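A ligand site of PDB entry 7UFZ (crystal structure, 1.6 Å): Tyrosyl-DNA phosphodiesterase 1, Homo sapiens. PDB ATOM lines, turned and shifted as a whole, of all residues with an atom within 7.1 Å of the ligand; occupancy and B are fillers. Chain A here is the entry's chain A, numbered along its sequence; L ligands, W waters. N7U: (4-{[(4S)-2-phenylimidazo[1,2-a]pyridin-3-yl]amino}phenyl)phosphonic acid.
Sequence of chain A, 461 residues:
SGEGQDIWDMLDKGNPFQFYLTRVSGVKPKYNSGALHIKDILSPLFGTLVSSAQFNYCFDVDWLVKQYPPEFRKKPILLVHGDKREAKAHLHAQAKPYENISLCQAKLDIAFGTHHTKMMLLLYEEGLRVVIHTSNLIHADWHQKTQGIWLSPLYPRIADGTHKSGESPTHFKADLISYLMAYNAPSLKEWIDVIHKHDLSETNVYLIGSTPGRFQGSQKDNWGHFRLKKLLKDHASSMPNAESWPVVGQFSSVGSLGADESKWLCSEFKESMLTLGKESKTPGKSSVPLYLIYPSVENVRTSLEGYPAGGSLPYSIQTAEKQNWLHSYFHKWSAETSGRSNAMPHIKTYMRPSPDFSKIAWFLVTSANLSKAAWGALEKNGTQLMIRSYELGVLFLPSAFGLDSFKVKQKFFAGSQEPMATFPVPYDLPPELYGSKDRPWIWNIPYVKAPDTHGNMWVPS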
ATOM      1  N   ASN A  56     -37.813   8.671  15.923  1.00  0.00           N
ATOM      2  CA  ASN A  56     -36.475   8.461  15.365  1.00  0.00           C
ATOM      3  C   ASN A  56     -35.425   9.174  16.214  1.00  0.00           C
ATOM      4  O   ASN A  56     -35.712   9.794  17.252  1.00  0.00           O
ATOM      5  CB  ASN A  56     -36.401   8.919  13.902  1.00  0.00           C
ATOM      6  CG  ASN A  56     -35.544   7.956  13.065  1.00  0.00           C
ATOM      7  OD1 ASN A  56     -34.326   7.890  13.241  1.00  0.00           O
ATOM      8  ND2 ASN A  56     -36.186   7.168  12.194  1.00  0.00           N
ATOM      9  N   TYR A  57     -34.178   9.117  15.725  1.00  0.00           N
ATOM     10  CA  TYR A  57     -33.051   9.820  16.336  1.00  0.00           C
ATOM     11  C   TYR A  57     -32.722  11.092  15.556  1.00  0.00           C
ATOM     12  O   TYR A  57     -32.731  12.202  16.111  1.00  0.00           O
ATOM     13  CB  TYR A  57     -31.840   8.871  16.406  1.00  0.00           C
ATOM     14  CG  TYR A  57     -30.603   9.575  16.926  1.00  0.00           C
ATOM     15  CD1 TYR A  57     -30.532   9.974  18.242  1.00  0.00           C
ATOM     16  CD2 TYR A  57     -29.532   9.841  16.086  1.00  0.00           C
ATOM     17  CE1 TYR A  57     -29.414  10.638  18.714  1.00  0.00           C
ATOM     18  CE2 TYR A  57     -28.408  10.492  16.567  1.00  0.00           C
ATOM     19  CZ  TYR A  57     -28.361  10.877  17.880  1.00  0.00           C
ATOM     20  OH  TYR A  57     -27.258  11.516  18.382  1.00  0.00           O
ATOM     21  N   CYS A  58     -32.431  10.959  14.254  1.00  0.00           N
ATOM     22  CA  CYS A  58     -32.012  12.053  13.378  1.00  0.00           C
ATOM     23  C   CYS A  58     -33.045  12.270  12.276  1.00  0.00           C
ATOM     24  O   CYS A  58     -33.496  11.302  11.645  1.00  0.00           O
ATOM     25  CB  CYS A  58     -30.607  11.746  12.739  1.00  0.00           C
ATOM     26  SG  CYS A  58     -29.907  13.149  11.868  1.00  0.00           S
ATOM     27  N   THR A 114     -30.158   8.313  24.973  1.00  0.00           N
ATOM     28  CA  THR A 114     -30.492   8.752  23.638  1.00  0.00           C
ATOM     29  C   THR A 114     -31.865   8.205  23.272  1.00  0.00           C
ATOM     30  O   THR A 114     -32.254   7.142  23.770  1.00  0.00           O
ATOM     31  CB  THR A 114     -29.449   8.222  22.646  1.00  0.00           C
ATOM     32  OG1 THR A 114     -28.163   8.739  22.987  1.00  0.00           O
ATOM     33  CG2 THR A 114     -29.773   8.668  21.259  1.00  0.00           C
ATOM     34  N   HIS A 115     -32.569   8.861  22.363  1.00  0.00           N
ATOM     35  CA  HIS A 115     -33.805   8.323  21.797  1.00  0.00           C
ATOM     36  C   HIS A 115     -33.488   7.691  20.441  1.00  0.00           C
ATOM     37  O   HIS A 115     -33.454   8.389  19.420  1.00  0.00           O
ATOM     38  CB  HIS A 115     -34.896   9.385  21.684  1.00  0.00           C
ATOM     39  CG  HIS A 115     -36.193   8.821  21.193  1.00  0.00           C
ATOM     40  ND1 HIS A 115     -36.530   8.711  19.863  1.00  0.00           N
ATOM     41  CD2 HIS A 115     -37.235   8.281  21.895  1.00  0.00           C
ATOM     42  CE1 HIS A 115     -37.721   8.151  19.755  1.00  0.00           C
ATOM     43  NE2 HIS A 115     -38.177   7.892  20.978  1.00  0.00           N
ATOM     44  N   HIS A 116     -33.306   6.366  20.423  1.00  0.00           N
ATOM     45  CA  HIS A 116     -32.853   5.679  19.219  1.00  0.00           C
ATOM     46  C   HIS A 116     -33.962   4.927  18.499  1.00  0.00           C
ATOM     47  O   HIS A 116     -33.758   4.530  17.351  1.00  0.00           O
ATOM     48  CB  HIS A 116     -31.735   4.674  19.509  1.00  0.00           C
ATOM     49  CG  HIS A 116     -30.389   5.281  19.672  1.00  0.00           C
ATOM     50  ND1 HIS A 116     -29.758   5.984  18.664  1.00  0.00           N
ATOM     51  CD2 HIS A 116     -29.530   5.275  20.724  1.00  0.00           C
ATOM     52  CE1 HIS A 116     -28.585   6.407  19.095  1.00  0.00           C
ATOM     53  NE2 HIS A 116     -28.420   5.982  20.340  1.00  0.00           N
ATOM     54  N   THR A 117     -35.094   4.681  19.146  1.00  0.00           N
ATOM     55  CA  THR A 117     -36.200   3.975  18.516  1.00  0.00           C
ATOM     56  C   THR A 117     -36.577   4.576  17.163  1.00  0.00           C
ATOM     57  O   THR A 117     -36.744   5.795  17.026  1.00  0.00           O
ATOM     58  CB  THR A 117     -37.393   4.042  19.436  1.00  0.00           C
ATOM     59  OG1 THR A 117     -37.073   3.321  20.621  1.00  0.00           O
ATOM     60  CG2 THR A 117     -38.697   3.566  18.790  1.00  0.00           C
ATOM     61  N   LYS A 118     -36.793   3.688  16.189  1.00  0.00           N
ATOM     62  CA  LYS A 118     -37.163   4.067  14.825  1.00  0.00           C
ATOM     63  C   LYS A 118     -38.464   3.341  14.520  1.00  0.00           C
ATOM     64  O   LYS A 118     -38.484   2.111  14.366  1.00  0.00           O
ATOM     65  CB  LYS A 118     -36.060   3.687  13.844  1.00  0.00           C
ATOM     66  CG  LYS A 118     -34.857   4.616  14.109  1.00  0.00           C
ATOM     67  CD  LYS A 118     -33.625   4.080  13.547  1.00  0.00           C
ATOM     68  CE  LYS A 118     -32.493   5.056  13.834  1.00  0.00           C
ATOM     69  NZ  LYS A 118     -32.012   4.868  15.196  1.00  0.00           N
ATOM     70  N   THR A 134     -34.890   0.413  11.154  1.00  0.00           N
ATOM     71  CA  THR A 134     -33.568   0.758  11.672  1.00  0.00           C
ATOM     72  C   THR A 134     -32.989   2.050  11.094  1.00  0.00           C
ATOM     73  O   THR A 134     -31.874   2.402  11.463  1.00  0.00           O
ATOM     74  CB  THR A 134     -32.556  -0.379  11.453  1.00  0.00           C
ATOM     75  OG1 THR A 134     -32.372  -0.616  10.043  1.00  0.00           O
ATOM     76  CG2 THR A 134     -33.064  -1.694  12.090  1.00  0.00           C
ATOM     77  N   SER A 135     -33.709   2.768  10.221  1.00  0.00           N
ATOM     78  CA  SER A 135     -33.125   3.900   9.504  1.00  0.00           C
ATOM     79  C   SER A 135     -33.465   5.233  10.142  1.00  0.00           C
ATOM     80  O   SER A 135     -34.628   5.490  10.474  1.00  0.00           O
ATOM     81  CB  SER A 135     -33.635   3.957   8.058  1.00  0.00           C
ATOM     82  OG  SER A 135     -33.338   2.747   7.378  1.00  0.00           O
ATOM     83  N   ASN A 136     -32.456   6.118  10.196  1.00  0.00           N
ATOM     84  CA  ASN A 136     -32.750   7.521  10.478  1.00  0.00           C
ATOM     85  C   ASN A 136     -33.532   8.125   9.317  1.00  0.00           C
ATOM     86  O   ASN A 136     -33.526   7.608   8.203  1.00  0.00           O
ATOM     87  CB  ASN A 136     -31.446   8.301  10.705  1.00  0.00           C
ATOM     88  CG  ASN A 136     -30.760   7.901  12.005  1.00  0.00           C
ATOM     89  OD1 ASN A 136     -31.143   8.375  13.054  1.00  0.00           O
ATOM     90  ND2 ASN A 136     -29.763   7.025  11.939  1.00  0.00           N
ATOM     91  N   ASP A 141     -29.428   7.390   4.990  1.00  0.00           N
ATOM     92  CA  ASP A 141     -29.722   6.130   5.640  1.00  0.00           C
ATOM     93  C   ASP A 141     -30.551   5.215   4.754  1.00  0.00           C
ATOM     94  O   ASP A 141     -30.573   3.999   5.001  1.00  0.00           O
ATOM     95  CB  ASP A 141     -30.447   6.348   6.985  1.00  0.00           C
ATOM     96  CG  ASP A 141     -29.496   6.340   8.157  1.00  0.00           C
ATOM     97  OD1 ASP A 141     -28.378   6.922   8.028  1.00  0.00           O
ATOM     98  OD2 ASP A 141     -29.852   5.775   9.221  1.00  0.00           O
ATOM     99  N   SER A 252     -24.072  -1.639  14.505  1.00  0.00           N
ATOM    100  CA  SER A 252     -23.326  -0.593  13.808  1.00  0.00           C
ATOM    101  C   SER A 252     -22.621   0.380  14.751  1.00  0.00           C
ATOM    102  O   SER A 252     -21.957   1.321  14.282  1.00  0.00           O
ATOM    103  CB  SER A 252     -24.270   0.123  12.831  1.00  0.00           C
ATOM    104  OG  SER A 252     -25.405   0.678  13.451  1.00  0.00           O
ATOM    105  N   SER A 253     -22.701   0.162  16.069  1.00  0.00           N
ATOM    106  CA  SER A 253     -22.026   0.997  17.041  1.00  0.00           C
ATOM    107  C   SER A 253     -21.719   0.137  18.252  1.00  0.00           C
ATOM    108  O   SER A 253     -22.433  -0.832  18.537  1.00  0.00           O
ATOM    109  CB  SER A 253     -22.907   2.196  17.433  1.00  0.00           C
ATOM    110  OG  SER A 253     -22.151   3.049  18.271  1.00  0.00           O
ATOM    111  N   VAL A 254     -20.652   0.502  18.943  1.00  0.00           N
ATOM    112  CA  VAL A 254     -20.150  -0.240  20.095  1.00  0.00           C
ATOM    113  C   VAL A 254     -19.958   0.748  21.247  1.00  0.00           C
ATOM    114  O   VAL A 254     -19.261   1.762  21.085  1.00  0.00           O
ATOM    115  CB  VAL A 254     -18.815  -0.920  19.769  1.00  0.00           C
ATOM    116  CG1 VAL A 254     -18.396  -1.818  20.919  1.00  0.00           C
ATOM    117  CG2 VAL A 254     -18.928  -1.701  18.464  1.00  0.00           C
ATOM    118  N   SER A 312     -21.690   6.750   9.920  1.00  0.00           N
ATOM    119  CA  SER A 312     -22.809   6.064  10.531  1.00  0.00           C
ATOM    120  C   SER A 312     -22.370   4.810  11.285  1.00  0.00           C
ATOM    121  O   SER A 312     -23.200   3.937  11.587  1.00  0.00           O
ATOM    122  CB  SER A 312     -23.846   5.716   9.465  1.00  0.00           C
ATOM    123  OG  SER A 312     -24.299   6.947   8.864  1.00  0.00           O
ATOM    124  N   LEU A 313     -21.082   4.709  11.593  1.00  0.00           N
ATOM    125  CA  LEU A 313     -20.528   3.567  12.351  1.00  0.00           C
ATOM    126  C   LEU A 313     -19.759   4.141  13.524  1.00  0.00           C
ATOM    127  O   LEU A 313     -18.521   4.160  13.534  1.00  0.00           O
ATOM    128  CB  LEU A 313     -19.640   2.685  11.474  1.00  0.00           C
ATOM    129  CG  LEU A 313     -20.407   1.926  10.361  1.00  0.00           C
ATOM    130  CD1 LEU A 313     -19.451   1.418   9.242  1.00  0.00           C
ATOM    131  CD2 LEU A 313     -21.205   0.700  10.863  1.00  0.00           C
ATOM    132  N   PRO A 314     -20.485   4.687  14.530  1.00  0.00           N
ATOM    133  CA  PRO A 314     -19.819   5.397  15.636  1.00  0.00           C
ATOM    134  C   PRO A 314     -19.168   4.412  16.588  1.00  0.00           C
ATOM    135  O   PRO A 314     -19.839   3.644  17.294  1.00  0.00           O
ATOM    136  CB  PRO A 314     -20.981   6.158  16.301  1.00  0.00           C
ATOM    137  CG  PRO A 314     -22.207   5.946  15.440  1.00  0.00           C
ATOM    138  CD  PRO A 314     -21.947   4.677  14.677  1.00  0.00           C
ATOM    139  N   HIS A 346     -26.535  -0.600   8.806  1.00  0.00           N
ATOM    140  CA  HIS A 346     -27.082   0.168   9.908  1.00  0.00           C
ATOM    141  C   HIS A 346     -28.242  -0.568  10.565  1.00  0.00           C
ATOM    142  O   HIS A 346     -28.726  -0.121  11.615  1.00  0.00           O
ATOM    143  CB  HIS A 346     -27.485   1.556   9.369  1.00  0.00           C
ATOM    144  CG  HIS A 346     -27.895   2.524  10.432  1.00  0.00           C
ATOM    145  ND1 HIS A 346     -29.214   2.702  10.797  1.00  0.00           N
ATOM    146  CD2 HIS A 346     -27.165   3.362  11.213  1.00  0.00           C
ATOM    147  CE1 HIS A 346     -29.279   3.607  11.759  1.00  0.00           C
ATOM    148  NE2 HIS A 346     -28.053   4.031  12.028  1.00  0.00           N
ATOM    149  N   LYS A 348     -29.538  -3.574  12.936  1.00  0.00           N
ATOM    150  CA  LYS A 348     -28.986  -4.352  14.044  1.00  0.00           C
ATOM    151  C   LYS A 348     -29.844  -5.589  14.161  1.00  0.00           C
ATOM    152  O   LYS A 348     -31.074  -5.501  14.104  1.00  0.00           O
ATOM    153  CB  LYS A 348     -29.000  -3.590  15.403  1.00  0.00           C
ATOM    154  CG  LYS A 348     -28.219  -2.241  15.374  1.00  0.00           C
ATOM    155  CD  LYS A 348     -29.058  -1.119  14.752  1.00  0.00           C
ATOM    156  CE  LYS A 348     -28.413   0.206  15.132  1.00  0.00           C
ATOM    157  NZ  LYS A 348     -28.381   1.160  13.989  1.00  0.00           N
ATOM    158  N   SER A 367     -33.304  -1.477  16.976  1.00  0.00           N
ATOM    159  CA  SER A 367     -32.432  -0.295  16.934  1.00  0.00           C
ATOM    160  C   SER A 367     -31.235  -0.459  17.861  1.00  0.00           C
ATOM    161  O   SER A 367     -30.283   0.325  17.786  1.00  0.00           O
ATOM    162  CB  SER A 367     -33.224   0.957  17.361  1.00  0.00           C
ATOM    163  OG  SER A 367     -33.774   0.750  18.696  1.00  0.00           O
ATOM    164  N   ALA A 368     -31.258  -1.459  18.752  1.00  0.00           N
ATOM    165  CA  ALA A 368     -30.248  -1.517  19.817  1.00  0.00           C
ATOM    166  C   ALA A 368     -28.884  -1.993  19.304  1.00  0.00           C
ATOM    167  O   ALA A 368     -28.743  -3.109  18.776  1.00  0.00           O
ATOM    168  CB  ALA A 368     -30.719  -2.436  20.945  1.00  0.00           C
ATOM    169  N   ASN A 369     -27.883  -1.135  19.479  1.00  0.00           N
ATOM    170  CA  ASN A 369     -26.480  -1.466  19.216  1.00  0.00           C
ATOM    171  C   ASN A 369     -25.881  -2.228  20.403  1.00  0.00           C
ATOM    172  O   ASN A 369     -26.572  -2.555  21.386  1.00  0.00           O
ATOM    173  CB  ASN A 369     -25.698  -0.181  18.958  1.00  0.00           C
ATOM    174  CG  ASN A 369     -25.885   0.307  17.534  1.00  0.00           C
ATOM    175  OD1 ASN A 369     -25.730  -0.462  16.596  1.00  0.00           O
ATOM    176  ND2 ASN A 369     -26.227   1.606  17.375  1.00  0.00           N
ATOM    177  N   GLU A 391     -35.093   2.247  22.880  1.00  0.00           N
ATOM    178  CA  GLU A 391     -34.792   1.352  21.761  1.00  0.00           C
ATOM    179  C   GLU A 391     -36.038   0.547  21.454  1.00  0.00           C
ATOM    180  O   GLU A 391     -36.879   0.360  22.330  1.00  0.00           O
ATOM    181  CB  GLU A 391     -33.676   0.358  22.079  1.00  0.00           C
ATOM    182  CG  GLU A 391     -32.427   0.998  22.663  1.00  0.00           C
ATOM    183  CD  GLU A 391     -31.532   1.592  21.568  1.00  0.00           C
ATOM    184  OE1 GLU A 391     -30.519   2.242  21.961  1.00  0.00           O
ATOM    185  OE2 GLU A 391     -31.845   1.442  20.373  1.00  0.00           O
ATOM    186  N   TRP A 443     -14.235   5.537  13.988  1.00  0.00           N
ATOM    187  CA  TRP A 443     -14.693   6.623  13.132  1.00  0.00           C
ATOM    188  C   TRP A 443     -13.963   7.938  13.335  1.00  0.00           C
ATOM    189  O   TRP A 443     -14.122   8.842  12.504  1.00  0.00           O
ATOM    190  CB  TRP A 443     -16.221   6.822  13.291  1.00  0.00           C
ATOM    191  CG  TRP A 443     -16.707   7.538  14.550  1.00  0.00           C
ATOM    192  CD1 TRP A 443     -16.057   7.646  15.747  1.00  0.00           C
ATOM    193  CD2 TRP A 443     -17.949   8.237  14.702  1.00  0.00           C
ATOM    194  NE1 TRP A 443     -16.827   8.364  16.639  1.00  0.00           N
ATOM    195  CE2 TRP A 443     -17.996   8.738  16.023  1.00  0.00           C
ATOM    196  CE3 TRP A 443     -19.033   8.473  13.854  1.00  0.00           C
ATOM    197  CZ2 TRP A 443     -19.067   9.482  16.507  1.00  0.00           C
ATOM    198  CZ3 TRP A 443     -20.105   9.203  14.339  1.00  0.00           C
ATOM    199  CH2 TRP A 443     -20.113   9.709  15.650  1.00  0.00           C
HETATM  200  C26 N7U L   1     -26.008   5.320  17.076  1.00  0.00           C
HETATM  201  C05 N7U L   1     -26.921   6.101  16.394  1.00  0.00           C
HETATM  202  C06 N7U L   1     -26.846   7.479  16.481  1.00  0.00           C
HETATM  203  C07 N7U L   1     -25.852   8.063  17.259  1.00  0.00           C
HETATM  204  C08 N7U L   1     -24.945   7.276  17.947  1.00  0.00           C
HETATM  205  C25 N7U L   1     -25.026   5.897  17.853  1.00  0.00           C
HETATM  206  N09 N7U L   1     -23.915   7.905  18.755  1.00  0.00           N
HETATM  207  O01 N7U L   1     -29.610   5.688  15.924  1.00  0.00           O
HETATM  208  O03 N7U L   1     -28.182   5.789  13.930  1.00  0.00           O
HETATM  209  O04 N7U L   1     -27.935   3.788  15.348  1.00  0.00           O
HETATM  210  P02 N7U L   1     -28.251   5.286  15.365  1.00  0.00           P
HETATM  211  O   HOH W   1     -30.191   2.665  16.618  1.00  0.00           O
HETATM  212  O   HOH W   2     -25.013   3.371  13.955  1.00  0.00           O
HETATM  213  O   HOH W   3     -26.710   3.341  19.381  1.00  0.00           O
HETATM  214  O   HOH W   4     -25.890   6.493  12.740  1.00  0.00           O
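The side-chain amide nitrogen (ND2) of Asn 369 is in hydrogen-bond range of an oxygen (O04) of the ligand (3.4 Å).
ND2 of Asn 136 is in hydrogen-bond range of O03 of the ligand (2.8 Å).
NZ of Lys 348 is in salt-bridge range of O04 of the ligand (3.0 Å).
O01 of the ligand lies within hydrogen-bond range of ND1 of His 116 (2.8 Å).
The side-chain amino group (NZ) of Lys 118 is in salt-bridge range of an oxygen (O01) of the ligand (2.6 Å).
A ring nitrogen (NE2) of His 346 lies within hydrogen-bond range of an oxygen (O03) of the ligand.
NZ of Lys 348 sits at hydrogen-bond distance from O of His 346 (2.7 Å).
O of His 116 sits at hydrogen-bond distance from NZ of Lys 118 (2.8 Å).
The backbone NH (N) of Ser 253 sits at hydrogen-bond distance from the side-chain amide oxygen (OD1) of Asn 369 (3.1 Å).
The backbone carbonyl oxygen of Pro 314 lies within hydrogen-bond range of the side-chain hydroxyl of Ser 253, at 2.6 Å.
ND1 of His 346 lies within hydrogen-bond range of O of Thr 134 (2.8 Å).
The side-chain amide oxygen (OD1) of Asn 136 sits close to the side-chain amide oxygen (OD1) of Asn 56 (3.2 Å).
The backbone NH (N) of Asn 136 is in hydrogen-bond range of the side-chain carboxylate (OD2) of Asp 141.
The backbone NH (N) of Cys 58 is in hydrogen-bond range of the side-chain amide oxygen (OD1) of Asn 136 (3.1 Å).
Merely in contact with the ligand: Tyr 57 (3.4 Å) and Pro 314 (3.7 Å).
Of the 25 residues printed, 8 come within 4 Å of the ligand.
The nearest printed residue that does not touch the ligand is Ser 253 (4.1 Å).
Water W4 lies within hydrogen-bond range of an oxygen (O03) of the ligand (2.7 Å) and a ring nitrogen (NE2) of His 346 (3.4 Å).
Water W1 lies within hydrogen-bond range of the backbone carbonyl oxygen of Ser 367 (2.6 Å), an oxygen (O04) of the ligand (2.8 Å) and the side-chain amino group of Lys 118 (3.2 Å).
Water W3 lies within hydrogen-bond range of the side-chain amide nitrogen of Asn 369 (2.7 Å) and a ring nitrogen (NE2) of His 116 (3.3 Å).
Water W2 lies within hydrogen-bond range of OG of Ser 252 (2.8 Å), O of Ser 312 (3.0 Å) and O04 of the ligand (3.3 Å).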
